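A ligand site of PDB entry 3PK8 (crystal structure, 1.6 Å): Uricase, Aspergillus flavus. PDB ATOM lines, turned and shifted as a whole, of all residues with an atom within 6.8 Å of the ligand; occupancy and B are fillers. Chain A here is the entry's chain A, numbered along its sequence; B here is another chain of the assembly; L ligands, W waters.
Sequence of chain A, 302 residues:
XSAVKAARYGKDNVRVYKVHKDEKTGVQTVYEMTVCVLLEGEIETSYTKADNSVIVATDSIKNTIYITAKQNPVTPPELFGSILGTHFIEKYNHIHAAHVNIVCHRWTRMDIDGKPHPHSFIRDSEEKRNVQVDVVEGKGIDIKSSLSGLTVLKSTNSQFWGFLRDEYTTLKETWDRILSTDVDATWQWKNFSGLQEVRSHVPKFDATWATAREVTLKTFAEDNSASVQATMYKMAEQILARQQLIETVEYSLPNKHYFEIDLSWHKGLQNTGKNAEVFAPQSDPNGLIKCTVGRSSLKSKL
Water W2 bridges N5 of the ligand and NH1 of Arg 177.
Water W1 bridges the side-chain hydroxyl (OG1) of Thr 58 of chain B (2.8 Å) and the side-chain amide nitrogen (ND2) of Asn 255 (3.0 Å).
Phe 160 touches the ligand (CE2 to C2, 3.4 Å).
Leu 171 touches the ligand.
Ser 227 touches the ligand.
CD2 of Tyr 9 of chain B touches O2 of the ligand (3.8 Å).
CG2 of Ile 55 of chain B touches O2 of the ligand, 3.6 Å away.
Ala 57 of chain B touches the ligand (CA to N3, 3.5 Å).
N of Asp 59 of chain B touches N4 of the ligand, 3.9 Å away.
Hydrophobic or aromatic side chains that line the ligand: Phe 160, Leu 171, Val 228, Tyr 9 of chain B, Ile 55 of chain B and Ala 57 of chain B.
12 residues have an atom within 4 Å of the ligand: Phe 160, Leu 171, Arg 177, Ser 227, Val 228, Gln 229, Asn 255, Tyr 9 of chain B, Ile 55 of chain B, Ala 57 of chain B, Thr 58 of chain B and Asp 59 of chain B.
The side-chain amino group of Lys 11 of chain B lies within hydrogen-bond range of the side-chain hydroxyl of Thr 58 of chain B.
N of Arg 177 sits at hydrogen-bond distance from O of Ser 158, 2.9 Å away.
OG of Ser 227 sits close to N of Gln 229 (3.4 Å).
O of Asn 255 sits at hydrogen-bond distance from NE2 of His 257.
N of Asn 255 lies within hydrogen-bond range of O of Gly 287, at 2.8 Å.
The side-chain hydroxyl (OG) of Ser 225 is in hydrogen-bond range of the backbone carbonyl oxygen (O) of Ser 227 (2.9 Å).
The backbone carbonyl oxygen of Val 56 of chain B is in hydrogen-bond range of the side-chain hydroxyl of Tyr 9 of chain B, 2.6 Å away.
N3 of the ligand sits at hydrogen-bond distance from N of Thr 58 of chain B (2.8 Å).
The side-chain hydroxyl (OG1) of Thr 58 of chain B sits at hydrogen-bond distance from a nitrogen (N3) of the ligand (3.2 Å).
The guanidinium group of Arg 177 is in hydrogen-bond range of an oxygen (O1) of the ligand (2.8 Å).
The side-chain amide nitrogen of Gln 229 lies within hydrogen-bond range of an oxygen (O2) of the ligand (2.9 Å).
The backbone NH (N) of Val 228 lies within hydrogen-bond range of an oxygen (O1) of the ligand, at 2.9 Å.
ND2 of Asn 255 sits close to N2 of the ligand, 3.3 Å away.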
ATOM      1  N   SER A 158      23.199  -0.048  -2.484  1.00  0.00           N
ATOM      2  CA  SER A 158      21.892  -0.659  -2.439  1.00  0.00           C
ATOM      3  C   SER A 158      21.496  -0.685  -0.969  1.00  0.00           C
ATOM      4  O   SER A 158      22.305  -1.006  -0.098  1.00  0.00           O
ATOM      5  CB  SER A 158      21.909  -2.073  -3.033  1.00  0.00           C
ATOM      6  OG  SER A 158      20.690  -2.743  -2.792  1.00  0.00           O
ATOM      7  N   GLN A 159      20.237  -0.331  -0.712  1.00  0.00           N
ATOM      8  CA  GLN A 159      19.688  -0.273   0.630  1.00  0.00           C
ATOM      9  C   GLN A 159      18.361  -0.991   0.647  1.00  0.00           C
ATOM     10  O   GLN A 159      17.710  -1.181  -0.378  1.00  0.00           O
ATOM     11  CB  GLN A 159      19.449   1.196   1.065  1.00  0.00           C
ATOM     12  CG  GLN A 159      20.633   2.109   0.799  1.00  0.00           C
ATOM     13  CD  GLN A 159      20.468   3.521   1.376  1.00  0.00           C
ATOM     14  OE1 GLN A 159      19.410   3.888   1.875  1.00  0.00           O
ATOM     15  NE2 GLN A 159      21.547   4.297   1.305  1.00  0.00           N
ATOM     16  N   PHE A 160      17.929  -1.369   1.844  1.00  0.00           N
ATOM     17  CA  PHE A 160      16.589  -1.880   2.015  1.00  0.00           C
ATOM     18  C   PHE A 160      16.153  -1.733   3.462  1.00  0.00           C
ATOM     19  O   PHE A 160      16.505  -2.533   4.333  1.00  0.00           O
ATOM     20  CB  PHE A 160      16.451  -3.344   1.505  1.00  0.00           C
ATOM     21  CG  PHE A 160      15.035  -3.796   1.396  1.00  0.00           C
ATOM     22  CD1 PHE A 160      14.159  -3.165   0.500  1.00  0.00           C
ATOM     23  CD2 PHE A 160      14.549  -4.824   2.195  1.00  0.00           C
ATOM     24  CE1 PHE A 160      12.832  -3.552   0.421  1.00  0.00           C
ATOM     25  CE2 PHE A 160      13.226  -5.227   2.110  1.00  0.00           C
ATOM     26  CZ  PHE A 160      12.346  -4.576   1.229  1.00  0.00           C
ATOM     27  N   PHE A 163      10.606  -1.440   5.486  1.00  0.00           N
ATOM     28  CA  PHE A 163       9.566  -2.410   5.125  1.00  0.00           C
ATOM     29  C   PHE A 163       8.690  -2.802   6.318  1.00  0.00           C
ATOM     30  O   PHE A 163       9.043  -2.535   7.473  1.00  0.00           O
ATOM     31  CB  PHE A 163      10.192  -3.670   4.486  1.00  0.00           C
ATOM     32  CG  PHE A 163      11.353  -4.235   5.258  1.00  0.00           C
ATOM     33  CD1 PHE A 163      12.645  -3.788   5.025  1.00  0.00           C
ATOM     34  CD2 PHE A 163      11.134  -5.230   6.228  1.00  0.00           C
ATOM     35  CE1 PHE A 163      13.733  -4.297   5.728  1.00  0.00           C
ATOM     36  CE2 PHE A 163      12.222  -5.757   6.948  1.00  0.00           C
ATOM     37  CZ  PHE A 163      13.505  -5.284   6.706  1.00  0.00           C
ATOM     38  N   LEU A 171      14.090 -10.217   9.111  1.00  0.00           N
ATOM     39  CA  LEU A 171      15.057  -9.474   8.286  1.00  0.00           C
ATOM     40  C   LEU A 171      15.449  -8.139   8.936  1.00  0.00           C
ATOM     41  O   LEU A 171      14.562  -7.328   9.296  1.00  0.00           O
ATOM     42  CB  LEU A 171      14.469  -9.206   6.901  1.00  0.00           C
ATOM     43  CG  LEU A 171      15.384  -8.488   5.875  1.00  0.00           C
ATOM     44  CD1 LEU A 171      16.607  -9.359   5.503  1.00  0.00           C
ATOM     45  CD2 LEU A 171      14.614  -8.116   4.618  1.00  0.00           C
ATOM     46  N   ARG A 177      24.103  -2.958   1.106  1.00  0.00           N
ATOM     47  CA  ARG A 177      24.103  -4.404   0.818  1.00  0.00           C
ATOM     48  C   ARG A 177      24.556  -4.637  -0.602  1.00  0.00           C
ATOM     49  O   ARG A 177      24.678  -3.711  -1.410  1.00  0.00           O
ATOM     50  CB  ARG A 177      22.701  -4.977   1.022  1.00  0.00           C
ATOM     51  CG  ARG A 177      21.678  -4.453   0.017  1.00  0.00           C
ATOM     52  CD  ARG A 177      20.304  -5.081   0.217  1.00  0.00           C
ATOM     53  NE  ARG A 177      19.407  -4.624  -0.874  1.00  0.00           N
ATOM     54  CZ  ARG A 177      18.195  -5.099  -1.118  1.00  0.00           C
ATOM     55  NH1 ARG A 177      17.633  -6.041  -0.345  1.00  0.00           N
ATOM     56  NH2 ARG A 177      17.512  -4.592  -2.147  1.00  0.00           N
ATOM     57  N   LEU A 179      23.720  -6.063  -4.291  1.00  0.00           N
ATOM     58  CA  LEU A 179      22.548  -6.297  -5.150  1.00  0.00           C
ATOM     59  C   LEU A 179      22.994  -6.989  -6.432  1.00  0.00           C
ATOM     60  O   LEU A 179      23.841  -6.483  -7.166  1.00  0.00           O
ATOM     61  CB  LEU A 179      21.810  -4.979  -5.463  1.00  0.00           C
ATOM     62  CG  LEU A 179      20.551  -5.077  -6.322  1.00  0.00           C
ATOM     63  CD1 LEU A 179      19.537  -5.990  -5.651  1.00  0.00           C
ATOM     64  CD2 LEU A 179      19.931  -3.677  -6.507  1.00  0.00           C
ATOM     65  N   SER A 225      20.060   2.512  -4.722  1.00  0.00           N
ATOM     66  CA  SER A 225      18.804   1.789  -4.810  1.00  0.00           C
ATOM     67  C   SER A 225      18.073   1.636  -3.479  1.00  0.00           C
ATOM     68  O   SER A 225      18.619   1.162  -2.488  1.00  0.00           O
ATOM     69  CB  SER A 225      19.092   0.417  -5.446  1.00  0.00           C
ATOM     70  OG  SER A 225      17.926  -0.379  -5.408  1.00  0.00           O
ATOM     71  N   ALA A 226      16.805   2.034  -3.468  1.00  0.00           N
ATOM     72  CA  ALA A 226      15.995   1.933  -2.266  1.00  0.00           C
ATOM     73  C   ALA A 226      15.361   0.552  -2.158  1.00  0.00           C
ATOM     74  O   ALA A 226      14.882   0.158  -1.092  1.00  0.00           O
ATOM     75  CB  ALA A 226      14.882   2.998  -2.307  1.00  0.00           C
ATOM     76  N   SER A 227      15.368  -0.163  -3.283  1.00  0.00           N
ATOM     77  CA  SER A 227      14.761  -1.511  -3.386  1.00  0.00           C
ATOM     78  C   SER A 227      14.882  -1.922  -4.844  1.00  0.00           C
ATOM     79  O   SER A 227      15.123  -1.090  -5.720  1.00  0.00           O
ATOM     80  CB  SER A 227      13.284  -1.555  -2.974  1.00  0.00           C
ATOM     81  OG  SER A 227      12.455  -0.797  -3.880  1.00  0.00           O
ATOM     82  N   VAL A 228      14.675  -3.214  -5.114  1.00  0.00           N
ATOM     83  CA  VAL A 228      14.664  -3.654  -6.495  1.00  0.00           C
ATOM     84  C   VAL A 228      13.482  -2.986  -7.216  1.00  0.00           C
ATOM     85  O   VAL A 228      13.608  -2.564  -8.356  1.00  0.00           O
ATOM     86  CB  VAL A 228      14.553  -5.197  -6.549  1.00  0.00           C
ATOM     87  CG1 VAL A 228      14.370  -5.668  -7.969  1.00  0.00           C
ATOM     88  CG2 VAL A 228      15.828  -5.791  -5.950  1.00  0.00           C
ATOM     89  N   GLN A 229      12.354  -2.921  -6.512  1.00  0.00           N
ATOM     90  CA  GLN A 229      11.117  -2.321  -7.030  1.00  0.00           C
ATOM     91  C   GLN A 229      11.386  -0.896  -7.542  1.00  0.00           C
ATOM     92  O   GLN A 229      11.002  -0.543  -8.676  1.00  0.00           O
ATOM     93  CB  GLN A 229      10.069  -2.251  -5.920  1.00  0.00           C
ATOM     94  CG  GLN A 229       9.407  -3.612  -5.555  1.00  0.00           C
ATOM     95  CD  GLN A 229      10.162  -4.428  -4.522  1.00  0.00           C
ATOM     96  OE1 GLN A 229      11.386  -4.288  -4.349  1.00  0.00           O
ATOM     97  NE2 GLN A 229       9.428  -5.306  -3.828  1.00  0.00           N
ATOM     98  N   ASN A 255      16.200 -11.483  -6.963  1.00  0.00           N
ATOM     99  CA  ASN A 255      17.104 -10.858  -6.034  1.00  0.00           C
ATOM    100  C   ASN A 255      18.024 -11.986  -5.557  1.00  0.00           C
ATOM    101  O   ASN A 255      17.589 -12.827  -4.799  1.00  0.00           O
ATOM    102  CB  ASN A 255      16.301 -10.190  -4.914  1.00  0.00           C
ATOM    103  CG  ASN A 255      17.158  -9.300  -4.007  1.00  0.00           C
ATOM    104  OD1 ASN A 255      18.370  -9.138  -4.219  1.00  0.00           O
ATOM    105  ND2 ASN A 255      16.532  -8.732  -2.975  1.00  0.00           N
ATOM    106  N   HIS A 257      20.665 -13.439  -3.475  1.00  0.00           N
ATOM    107  CA  HIS A 257      21.133 -12.981  -2.165  1.00  0.00           C
ATOM    108  C   HIS A 257      22.568 -13.388  -1.872  1.00  0.00           C
ATOM    109  O   HIS A 257      22.971 -14.519  -2.168  1.00  0.00           O
ATOM    110  CB  HIS A 257      20.226 -13.494  -1.058  1.00  0.00           C
ATOM    111  CG  HIS A 257      18.783 -13.162  -1.263  1.00  0.00           C
ATOM    112  ND1 HIS A 257      18.303 -11.873  -1.174  1.00  0.00           N
ATOM    113  CD2 HIS A 257      17.719 -13.949  -1.557  1.00  0.00           C
ATOM    114  CE1 HIS A 257      16.988 -11.876  -1.389  1.00  0.00           C
ATOM    115  NE2 HIS A 257      16.619 -13.123  -1.637  1.00  0.00           N
ATOM    116  N   GLY A 287      14.481 -13.788  -3.991  1.00  0.00           N
ATOM    117  CA  GLY A 287      13.362 -12.874  -4.236  1.00  0.00           C
ATOM    118  C   GLY A 287      13.073 -12.846  -5.730  1.00  0.00           C
ATOM    119  O   GLY A 287      13.952 -13.085  -6.561  1.00  0.00           O
ATOM    120  N   ILE A 289      10.901 -10.235  -8.327  1.00  0.00           N
ATOM    121  CA  ILE A 289      10.158  -8.975  -8.358  1.00  0.00           C
ATOM    122  C   ILE A 289       9.782  -8.669  -9.793  1.00  0.00           C
ATOM    123  O   ILE A 289      10.643  -8.683 -10.674  1.00  0.00           O
ATOM    124  CB  ILE A 289      11.037  -7.788  -7.820  1.00  0.00           C
ATOM    125  CG1 ILE A 289      11.850  -8.187  -6.567  1.00  0.00           C
ATOM    126  CG2 ILE A 289      10.149  -6.532  -7.583  1.00  0.00           C
ATOM    127  CD1 ILE A 289      11.077  -8.566  -5.403  1.00  0.00           C
ATOM    128  N   TYR B   9       5.314  -9.656  -6.605  1.00  0.00           N
ATOM    129  CA  TYR B   9       6.668  -9.880  -6.096  1.00  0.00           C
ATOM    130  C   TYR B   9       6.532 -10.939  -4.991  1.00  0.00           C
ATOM    131  O   TYR B   9       5.455 -11.134  -4.425  1.00  0.00           O
ATOM    132  CB  TYR B   9       7.290  -8.560  -5.584  1.00  0.00           C
ATOM    133  CG  TYR B   9       6.826  -8.288  -4.177  1.00  0.00           C
ATOM    134  CD1 TYR B   9       5.516  -7.884  -3.936  1.00  0.00           C
ATOM    135  CD2 TYR B   9       7.649  -8.546  -3.096  1.00  0.00           C
ATOM    136  CE1 TYR B   9       5.059  -7.709  -2.623  1.00  0.00           C
ATOM    137  CE2 TYR B   9       7.219  -8.367  -1.796  1.00  0.00           C
ATOM    138  CZ  TYR B   9       5.905  -7.956  -1.578  1.00  0.00           C
ATOM    139  OH  TYR B   9       5.467  -7.816  -0.296  1.00  0.00           O
ATOM    140  N   GLY B  10       7.638 -11.608  -4.689  1.00  0.00           N
ATOM    141  CA  GLY B  10       7.646 -12.582  -3.616  1.00  0.00           C
ATOM    142  C   GLY B  10       8.916 -13.407  -3.594  1.00  0.00           C
ATOM    143  O   GLY B  10       9.976 -12.921  -3.907  1.00  0.00           O
ATOM    144  N   LYS B  11       8.789 -14.661  -3.184  1.00  0.00           N
ATOM    145  CA  LYS B  11       9.969 -15.522  -3.000  1.00  0.00           C
ATOM    146  C   LYS B  11       9.805 -16.749  -3.859  1.00  0.00           C
ATOM    147  O   LYS B  11       8.725 -17.384  -3.876  1.00  0.00           O
ATOM    148  CB  LYS B  11      10.114 -15.946  -1.530  1.00  0.00           C
ATOM    149  CG  LYS B  11      11.539 -16.390  -1.152  1.00  0.00           C
ATOM    150  CD  LYS B  11      12.527 -15.229  -1.283  1.00  0.00           C
ATOM    151  CE  LYS B  11      13.311 -14.965  -0.023  1.00  0.00           C
ATOM    152  NZ  LYS B  11      14.069 -13.679  -0.082  1.00  0.00           N
ATOM    153  N   ASN B  52       8.683   1.707   1.048  1.00  0.00           N
ATOM    154  CA  ASN B  52       8.776   0.303   1.438  1.00  0.00           C
ATOM    155  C   ASN B  52       7.748  -0.132   2.490  1.00  0.00           C
ATOM    156  O   ASN B  52       7.652  -1.309   2.822  1.00  0.00           O
ATOM    157  CB  ASN B  52      10.216  -0.036   1.866  1.00  0.00           C
ATOM    158  CG  ASN B  52      11.203   0.018   0.696  1.00  0.00           C
ATOM    159  OD1 ASN B  52      10.809  -0.116  -0.460  1.00  0.00           O
ATOM    160  ND2 ASN B  52      12.475   0.199   1.001  1.00  0.00           N
ATOM    161  N   ILE B  55       5.618  -3.070   1.672  1.00  0.00           N
ATOM    162  CA  ILE B  55       6.263  -4.344   1.311  1.00  0.00           C
ATOM    163  C   ILE B  55       6.348  -5.318   2.487  1.00  0.00           C
ATOM    164  O   ILE B  55       6.987  -5.027   3.500  1.00  0.00           O
ATOM    165  CB  ILE B  55       7.677  -4.138   0.763  1.00  0.00           C
ATOM    166  CG1 ILE B  55       7.637  -3.301  -0.517  1.00  0.00           C
ATOM    167  CG2 ILE B  55       8.343  -5.527   0.459  1.00  0.00           C
ATOM    168  CD1 ILE B  55       9.041  -2.889  -1.015  1.00  0.00           C
ATOM    169  N   VAL B  56       5.681  -6.454   2.327  1.00  0.00           N
ATOM    170  CA  VAL B  56       5.903  -7.622   3.173  1.00  0.00           C
ATOM    171  C   VAL B  56       7.214  -8.195   2.618  1.00  0.00           C
ATOM    172  O   VAL B  56       7.224  -8.623   1.452  1.00  0.00           O
ATOM    173  CB  VAL B  56       4.735  -8.612   3.063  1.00  0.00           C
ATOM    174  CG1 VAL B  56       5.039  -9.904   3.832  1.00  0.00           C
ATOM    175  CG2 VAL B  56       3.438  -7.950   3.620  1.00  0.00           C
ATOM    176  N   ALA B  57       8.311  -8.164   3.388  1.00  0.00           N
ATOM    177  CA  ALA B  57       9.632  -8.552   2.825  1.00  0.00           C
ATOM    178  C   ALA B  57       9.572  -9.984   2.292  1.00  0.00           C
ATOM    179  O   ALA B  57       8.874 -10.833   2.850  1.00  0.00           O
ATOM    180  CB  ALA B  57      10.752  -8.403   3.871  1.00  0.00           C
ATOM    181  N   THR B  58      10.315 -10.225   1.214  1.00  0.00           N
ATOM    182  CA  THR B  58      10.300 -11.554   0.604  1.00  0.00           C
ATOM    183  C   THR B  58      10.884 -12.545   1.604  1.00  0.00           C
ATOM    184  O   THR B  58      10.442 -13.691   1.673  1.00  0.00           O
ATOM    185  CB  THR B  58      11.064 -11.619  -0.741  1.00  0.00           C
ATOM    186  OG1 THR B  58      12.454 -11.398  -0.536  1.00  0.00           O
ATOM    187  CG2 THR B  58      10.502 -10.567  -1.740  1.00  0.00           C
ATOM    188  N   ASP B  59      11.845 -12.079   2.415  1.00  0.00           N
ATOM    189  CA  ASP B  59      12.373 -12.893   3.517  1.00  0.00           C
ATOM    190  C   ASP B  59      11.275 -13.352   4.484  1.00  0.00           C
ATOM    191  O   ASP B  59      11.286 -14.481   4.966  1.00  0.00           O
ATOM    192  CB  ASP B  59      13.470 -12.150   4.276  1.00  0.00           C
ATOM    193  CG  ASP B  59      14.211 -13.050   5.252  1.00  0.00           C
ATOM    194  OD1 ASP B  59      15.104 -13.808   4.811  1.00  0.00           O
ATOM    195  OD2 ASP B  59      13.888 -13.016   6.459  1.00  0.00           O
ATOM    196  N   SER B  60      10.322 -12.451   4.776  1.00  0.00           N
ATOM    197  CA  SER B  60       9.176 -12.800   5.625  1.00  0.00           C
ATOM    198  C   SER B  60       8.226 -13.789   4.973  1.00  0.00           C
ATOM    199  O   SER B  60       7.629 -14.630   5.662  1.00  0.00           O
ATOM    200  CB  SER B  60       8.411 -11.520   6.041  1.00  0.00           C
ATOM    201  OG  SER B  60       9.324 -10.601   6.601  1.00  0.00           O
HETATM  202  N1  LIG L   1      12.830  -5.904  -2.318  1.00  0.00           N
HETATM  203  C1  LIG L   1      14.170  -5.839  -2.124  1.00  0.00           C
HETATM  204  O1  LIG L   1      14.813  -5.054  -2.859  1.00  0.00           O
HETATM  205  N2  LIG L   1      14.832  -6.548  -1.155  1.00  0.00           N
HETATM  206  C2  LIG L   1      14.078  -7.332  -0.364  1.00  0.00           C
HETATM  207  C3  LIG L   1      12.657  -7.471  -0.522  1.00  0.00           C
HETATM  208  C4  LIG L   1      12.021  -6.679  -1.592  1.00  0.00           C
HETATM  209  O2  LIG L   1      10.796  -6.767  -1.793  1.00  0.00           O
HETATM  210  N3  LIG L   1      12.163  -8.348   0.418  1.00  0.00           N
HETATM  211  N4  LIG L   1      13.312  -8.721   1.128  1.00  0.00           N
HETATM  212  N5  LIG L   1      14.503  -8.121   0.669  1.00  0.00           N
HETATM  213  O   HOH W   1      13.942 -10.070  -2.470  1.00  0.00           O
HETATM  214  O   HOH W   2      16.983  -8.876   1.382  1.00  0.00           O
